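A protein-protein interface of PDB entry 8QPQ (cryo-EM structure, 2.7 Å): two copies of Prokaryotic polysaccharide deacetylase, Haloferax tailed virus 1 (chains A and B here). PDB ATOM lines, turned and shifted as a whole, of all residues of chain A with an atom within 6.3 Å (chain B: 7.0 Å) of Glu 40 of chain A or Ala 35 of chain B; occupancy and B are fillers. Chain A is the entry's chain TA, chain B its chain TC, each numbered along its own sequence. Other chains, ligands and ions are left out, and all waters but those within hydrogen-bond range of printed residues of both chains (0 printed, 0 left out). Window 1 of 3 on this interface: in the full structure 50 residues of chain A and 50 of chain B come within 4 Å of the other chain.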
ATOM      1  N   ARG A  38     -22.638  16.508   5.349  1.00  0.00           N
ATOM      2  CA  ARG A  38     -22.495  17.828   5.939  1.00  0.00           C
ATOM      3  C   ARG A  38     -23.638  18.104   6.911  1.00  0.00           C
ATOM      4  O   ARG A  38     -24.807  17.893   6.598  1.00  0.00           O
ATOM      5  CB  ARG A  38     -22.609  18.894   4.849  1.00  0.00           C
ATOM      6  CG  ARG A  38     -21.437  18.978   3.881  1.00  0.00           C
ATOM      7  CD  ARG A  38     -21.956  19.618   2.612  1.00  0.00           C
ATOM      8  NE  ARG A  38     -21.007  20.437   1.895  1.00  0.00           N
ATOM      9  CZ  ARG A  38     -21.280  21.232   0.875  1.00  0.00           C
ATOM     10  NH1 ARG A  38     -20.292  21.900   0.312  1.00  0.00           N
ATOM     11  NH2 ARG A  38     -22.508  21.391   0.417  1.00  0.00           N
ATOM     12  N   ILE A  39     -23.293  18.658   8.080  1.00  0.00           N
ATOM     13  CA  ILE A  39     -24.296  19.234   8.962  1.00  0.00           C
ATOM     14  C   ILE A  39     -24.325  20.740   8.736  1.00  0.00           C
ATOM     15  O   ILE A  39     -25.349  21.301   8.353  1.00  0.00           O
ATOM     16  CB  ILE A  39     -24.041  18.866  10.434  1.00  0.00           C
ATOM     17  CG1 ILE A  39     -23.977  17.344  10.603  1.00  0.00           C
ATOM     18  CG2 ILE A  39     -25.070  19.505  11.361  1.00  0.00           C
ATOM     19  CD1 ILE A  39     -25.176  16.592  10.079  1.00  0.00           C
ATOM     20  N   GLU A  40     -23.178  21.392   8.931  1.00  0.00           N
ATOM     21  CA  GLU A  40     -23.079  22.810   8.640  1.00  0.00           C
ATOM     22  C   GLU A  40     -22.863  22.988   7.144  1.00  0.00           C
ATOM     23  O   GLU A  40     -21.904  22.462   6.603  1.00  0.00           O
ATOM     24  CB  GLU A  40     -21.962  23.458   9.425  1.00  0.00           C
ATOM     25  CG  GLU A  40     -22.235  23.544  10.910  1.00  0.00           C
ATOM     26  CD  GLU A  40     -21.264  24.420  11.687  1.00  0.00           C
ATOM     27  OE1 GLU A  40     -20.032  24.316  11.460  1.00  0.00           O
ATOM     28  OE2 GLU A  40     -21.732  25.206  12.548  1.00  0.00           O
ATOM     29  N   ILE A  41     -23.753  23.739   6.487  1.00  0.00           N
ATOM     30  CA  ILE A  41     -23.616  24.012   5.066  1.00  0.00           C
ATOM     31  C   ILE A  41     -22.803  25.288   4.857  1.00  0.00           C
ATOM     32  O   ILE A  41     -22.905  26.245   5.619  1.00  0.00           O
ATOM     33  CB  ILE A  41     -24.991  24.048   4.366  1.00  0.00           C
ATOM     34  CG1 ILE A  41     -25.870  25.209   4.843  1.00  0.00           C
ATOM     35  CG2 ILE A  41     -25.680  22.698   4.510  1.00  0.00           C
ATOM     36  CD1 ILE A  41     -27.034  25.497   3.933  1.00  0.00           C
ATOM     37  N   PRO A  42     -21.959  25.349   3.811  1.00  0.00           N
ATOM     38  CA  PRO A  42     -21.161  26.546   3.557  1.00  0.00           C
ATOM     39  C   PRO A  42     -21.992  27.758   3.114  1.00  0.00           C
ATOM     40  O   PRO A  42     -21.665  28.884   3.481  1.00  0.00           O
ATOM     41  CB  PRO A  42     -20.117  26.032   2.553  1.00  0.00           C
ATOM     42  CG  PRO A  42     -20.835  24.939   1.793  1.00  0.00           C
ATOM     43  CD  PRO A  42     -21.708  24.278   2.837  1.00  0.00           C
ATOM     44  N   GLU A 282     -32.065  24.157  17.537  1.00  0.00           N
ATOM     45  CA  GLU A 282     -30.828  23.889  16.816  1.00  0.00           C
ATOM     46  C   GLU A 282     -30.398  22.428  16.962  1.00  0.00           C
ATOM     47  O   GLU A 282     -30.034  21.799  15.968  1.00  0.00           O
ATOM     48  CB  GLU A 282     -29.735  24.839  17.283  1.00  0.00           C
ATOM     49  CG  GLU A 282     -28.476  24.727  16.453  1.00  0.00           C
ATOM     50  CD  GLU A 282     -27.444  25.794  16.786  1.00  0.00           C
ATOM     51  OE1 GLU A 282     -27.227  26.056  17.988  1.00  0.00           O
ATOM     52  OE2 GLU A 282     -26.851  26.364  15.846  1.00  0.00           O
ATOM     53  N   LYS A 289     -31.169  16.457  10.634  1.00  0.00           N
ATOM     54  CA  LYS A 289     -30.276  16.395   9.483  1.00  0.00           C
ATOM     55  C   LYS A 289     -29.464  15.095   9.483  1.00  0.00           C
ATOM     56  O   LYS A 289     -29.523  14.354   8.511  1.00  0.00           O
ATOM     57  CB  LYS A 289     -29.440  17.674   9.400  1.00  0.00           C
ATOM     58  CG  LYS A 289     -28.730  17.897   8.070  1.00  0.00           C
ATOM     59  CD  LYS A 289     -28.217  19.317   7.873  1.00  0.00           C
ATOM     60  CE  LYS A 289     -27.416  19.470   6.583  1.00  0.00           C
ATOM     61  NZ  LYS A 289     -28.180  20.177   5.528  1.00  0.00           N
ATOM     62  N   ASN A 322     -27.220  28.163   9.021  1.00  0.00           N
ATOM     63  CA  ASN A 322     -25.997  27.382   9.133  1.00  0.00           C
ATOM     64  C   ASN A 322     -26.180  25.957   8.601  1.00  0.00           C
ATOM     65  O   ASN A 322     -25.199  25.283   8.312  1.00  0.00           O
ATOM     66  CB  ASN A 322     -25.495  27.366  10.575  1.00  0.00           C
ATOM     67  CG  ASN A 322     -25.214  28.751  11.120  1.00  0.00           C
ATOM     68  OD1 ASN A 322     -24.133  29.301  10.914  1.00  0.00           O
ATOM     69  ND2 ASN A 322     -26.186  29.324  11.812  1.00  0.00           N
ATOM     70  N   TYR A 323     -27.432  25.476   8.488  1.00  0.00           N
ATOM     71  CA  TYR A 323     -27.753  24.066   8.262  1.00  0.00           C
ATOM     72  C   TYR A 323     -28.586  23.844   6.993  1.00  0.00           C
ATOM     73  O   TYR A 323     -28.491  22.785   6.368  1.00  0.00           O
ATOM     74  CB  TYR A 323     -28.459  23.485   9.496  1.00  0.00           C
ATOM     75  CG  TYR A 323     -27.738  23.807  10.782  1.00  0.00           C
ATOM     76  CD1 TYR A 323     -26.526  23.194  11.084  1.00  0.00           C
ATOM     77  CD2 TYR A 323     -28.225  24.770  11.663  1.00  0.00           C
ATOM     78  CE1 TYR A 323     -25.817  23.534  12.227  1.00  0.00           C
ATOM     79  CE2 TYR A 323     -27.518  25.121  12.808  1.00  0.00           C
ATOM     80  CZ  TYR A 323     -26.308  24.503  13.085  1.00  0.00           C
ATOM     81  OH  TYR A 323     -25.573  24.841  14.185  1.00  0.00           O
ATOM     82  N   ARG B  32     -20.306  13.106  10.332  1.00  0.00           N
ATOM     83  CA  ARG B  32     -21.049  14.362  10.345  1.00  0.00           C
ATOM     84  C   ARG B  32     -20.100  15.551  10.456  1.00  0.00           C
ATOM     85  O   ARG B  32     -19.365  15.702  11.430  1.00  0.00           O
ATOM     86  CB  ARG B  32     -22.216  14.385  11.346  1.00  0.00           C
ATOM     87  CG  ARG B  32     -22.147  13.457  12.547  1.00  0.00           C
ATOM     88  CD  ARG B  32     -23.440  13.615  13.333  1.00  0.00           C
ATOM     89  NE  ARG B  32     -23.576  12.829  14.548  1.00  0.00           N
ATOM     90  CZ  ARG B  32     -23.970  11.560  14.607  1.00  0.00           C
ATOM     91  NH1 ARG B  32     -24.062  10.958  15.776  1.00  0.00           N
ATOM     92  NH2 ARG B  32     -24.225  10.892  13.494  1.00  0.00           N
ATOM     93  N   LEU B  33     -20.135  16.402   9.424  1.00  0.00           N
ATOM     94  CA  LEU B  33     -19.150  17.457   9.260  1.00  0.00           C
ATOM     95  C   LEU B  33     -19.728  18.831   9.615  1.00  0.00           C
ATOM     96  O   LEU B  33     -20.713  19.286   9.026  1.00  0.00           O
ATOM     97  CB  LEU B  33     -18.623  17.387   7.825  1.00  0.00           C
ATOM     98  CG  LEU B  33     -17.525  18.387   7.466  1.00  0.00           C
ATOM     99  CD1 LEU B  33     -16.231  18.078   8.199  1.00  0.00           C
ATOM    100  CD2 LEU B  33     -17.291  18.419   5.967  1.00  0.00           C
ATOM    101  N   TYR B  34     -19.068  19.506  10.570  1.00  0.00           N
ATOM    102  CA  TYR B  34     -19.374  20.869  10.967  1.00  0.00           C
ATOM    103  C   TYR B  34     -18.215  21.755  10.503  1.00  0.00           C
ATOM    104  O   TYR B  34     -17.363  22.150  11.296  1.00  0.00           O
ATOM    105  CB  TYR B  34     -19.621  20.933  12.477  1.00  0.00           C
ATOM    106  CG  TYR B  34     -20.689  20.025  13.035  1.00  0.00           C
ATOM    107  CD1 TYR B  34     -20.518  18.647  13.102  1.00  0.00           C
ATOM    108  CD2 TYR B  34     -21.847  20.557  13.588  1.00  0.00           C
ATOM    109  CE1 TYR B  34     -21.496  17.822  13.638  1.00  0.00           C
ATOM    110  CE2 TYR B  34     -22.826  19.746  14.148  1.00  0.00           C
ATOM    111  CZ  TYR B  34     -22.650  18.371  14.170  1.00  0.00           C
ATOM    112  OH  TYR B  34     -23.590  17.536  14.707  1.00  0.00           O
ATOM    113  N   ALA B  35     -18.190  22.039   9.196  1.00  0.00           N
ATOM    114  CA  ALA B  35     -17.079  22.749   8.579  1.00  0.00           C
ATOM    115  C   ALA B  35     -17.575  23.646   7.442  1.00  0.00           C
ATOM    116  O   ALA B  35     -17.150  23.510   6.293  1.00  0.00           O
ATOM    117  CB  ALA B  35     -16.031  21.750   8.132  1.00  0.00           C
ATOM    118  N   GLN B  36     -18.442  24.612   7.778  1.00  0.00           N
ATOM    119  CA  GLN B  36     -18.999  25.532   6.794  1.00  0.00           C
ATOM    120  C   GLN B  36     -17.930  26.460   6.207  1.00  0.00           C
ATOM    121  O   GLN B  36     -18.007  26.855   5.040  1.00  0.00           O
ATOM    122  CB  GLN B  36     -20.206  26.286   7.353  1.00  0.00           C
ATOM    123  CG  GLN B  36     -19.951  27.129   8.599  1.00  0.00           C
ATOM    124  CD  GLN B  36     -21.187  27.814   9.132  1.00  0.00           C
ATOM    125  OE1 GLN B  36     -22.278  27.719   8.567  1.00  0.00           O
ATOM    126  NE2 GLN B  36     -21.023  28.524  10.236  1.00  0.00           N
ATOM    127  N   ASP B  37     -16.892  26.754   6.994  1.00  0.00           N
ATOM    128  CA  ASP B  37     -15.840  27.690   6.623  1.00  0.00           C
ATOM    129  C   ASP B  37     -14.702  26.993   5.874  1.00  0.00           C
ATOM    130  O   ASP B  37     -13.661  26.666   6.451  1.00  0.00           O
ATOM    131  CB  ASP B  37     -15.416  28.461   7.869  1.00  0.00           C
ATOM    132  CG  ASP B  37     -16.539  29.290   8.472  1.00  0.00           C
ATOM    133  OD1 ASP B  37     -17.309  29.866   7.682  1.00  0.00           O
ATOM    134  OD2 ASP B  37     -16.641  29.345   9.721  1.00  0.00           O
ATOM    135  N   ARG B  38     -14.902  26.827   4.562  1.00  0.00           N
ATOM    136  CA  ARG B  38     -13.864  26.351   3.663  1.00  0.00           C
ATOM    137  C   ARG B  38     -12.832  27.452   3.432  1.00  0.00           C
ATOM    138  O   ARG B  38     -13.171  28.585   3.100  1.00  0.00           O
ATOM    139  CB  ARG B  38     -14.457  26.036   2.289  1.00  0.00           C
ATOM    140  CG  ARG B  38     -15.388  24.835   2.237  1.00  0.00           C
ATOM    141  CD  ARG B  38     -16.324  25.033   1.057  1.00  0.00           C
ATOM    142  NE  ARG B  38     -16.727  23.780   0.456  1.00  0.00           N
ATOM    143  CZ  ARG B  38     -17.358  23.634  -0.696  1.00  0.00           C
ATOM    144  NH1 ARG B  38     -17.642  22.415  -1.107  1.00  0.00           N
ATOM    145  NH2 ARG B  38     -17.688  24.666  -1.448  1.00  0.00           N
ATOM    146  N   ARG B 298     -19.981  34.272   4.323  1.00  0.00           N
ATOM    147  CA  ARG B 298     -20.067  32.859   3.965  1.00  0.00           C
ATOM    148  C   ARG B 298     -19.985  32.583   2.458  1.00  0.00           C
ATOM    149  O   ARG B 298     -19.738  33.480   1.655  1.00  0.00           O
ATOM    150  CB  ARG B 298     -21.188  32.153   4.742  1.00  0.00           C
ATOM    151  CG  ARG B 298     -20.725  31.647   6.100  1.00  0.00           C
ATOM    152  CD  ARG B 298     -21.529  30.425   6.557  1.00  0.00           C
ATOM    153  NE  ARG B 298     -22.838  30.817   7.034  1.00  0.00           N
ATOM    154  CZ  ARG B 298     -23.962  30.117   6.882  1.00  0.00           C
ATOM    155  NH1 ARG B 298     -25.093  30.592   7.371  1.00  0.00           N
ATOM    156  NH2 ARG B 298     -23.955  28.977   6.217  1.00  0.00           N
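The backbone carbonyl oxygen of Leu 33 of chain B is in hydrogen-bond range of the backbone NH of Ile 39 of chain A (2.8 Å). The backbone carbonyl oxygen (O) of Leu 33 of chain B sits at hydrogen-bond distance from the backbone NH (N) of Glu 40 of chain A. OE1 of Gln 36 of chain B sits close to O of Ile 41 of chain A (3.4 Å). NE2 of Gln 36 of chain B lies within hydrogen-bond range of OD1 of Asn 322 of chain A, at 3.3 Å. O of Ile 41 of chain A sits at hydrogen-bond distance from NH2 of Arg 298 of chain B, at 3.0 Å. NH1 of Arg 38 of chain A lies close to NH1 of Arg 38 of chain B (3.0 Å). OE1 of Glu 40 of chain A lies close to O of Tyr 34 of chain B (3.4 Å).
OE1 of Gln 36 of chain B lies within hydrogen-bond range of NH2 of Arg 298 of chain B (3.1 Å). The backbone NH (N) of Ile 41 of chain A sits at hydrogen-bond distance from the backbone carbonyl oxygen (O) of Asn 322 of chain A (2.8 Å).
Among the printed residues, pairs that only touch across the chains: Pro 42 of chain A with Gln 36 of chain B (3.4 Å), Pro 42 of chain A with Arg 298 of chain B (3.4 Å), Ile 39 of chain A with Arg 32 of chain B (3.5 Å), Ile 39 of chain A with Tyr 34 of chain B (3.6 Å), Asn 322 of chain A with Arg 298 of chain B (3.6 Å), Glu 40 of chain A with Ala 35 of chain B (3.7 Å), Arg 38 of chain A with Leu 33 of chain B (3.8 Å) and Glu 40 of chain A with Gln 36 of chain B (3.9 Å).
Ala 35 of chain B touches just one residue of chain A: Glu 40 (3.7 Å). Printed residues of chain B within 4 Å of Ile 39 of chain A: Arg 32, Leu 33 and Tyr 34. Of the printed residues of chain A, Tyr 34 of chain B touches Ile 39 and Glu 40. Of the printed residues of chain A, Arg 298 of chain B touches Ile 41 (3.0 Å), Pro 42 (3.4 Å) and Asn 322 (3.6 Å). Of the printed residues of chain B, Arg 38 of chain A touches Leu 33 and Arg 38. Glu 282 of chain A touches none of the printed residues of chain B. The nearest residue of chain A that does not touch Ala 35 of chain B is Pro 42 of chain A (5.4 Å). The nearest printed residue of chain A that does not touch Tyr 34 of chain B is Tyr 323 of chain A (5.1 Å).
Of the 8 printed residues of chain B, 7 touch a printed residue of chain A. Along chain B the printed residues that touch a printed residue of chain A span positions 32 to 298. Of the 9 printed residues of chain A, 6 touch a printed residue of chain B. Hydrophobic or aromatic side chains of chain A within 4 Å of the printed part of chain B: Ile 39 and Pro 42. Among the printed residues, no Asp or Glu carboxylate lies within 4 Å of a Lys or Arg side-chain nitrogen of the other chain.
Arg 38 of chain A touches its own counterpart, Arg 38 of chain B. Of the 15 pairs that touch across the chains among the printed residues, 1 has its exchanged pair printed and touching as well.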
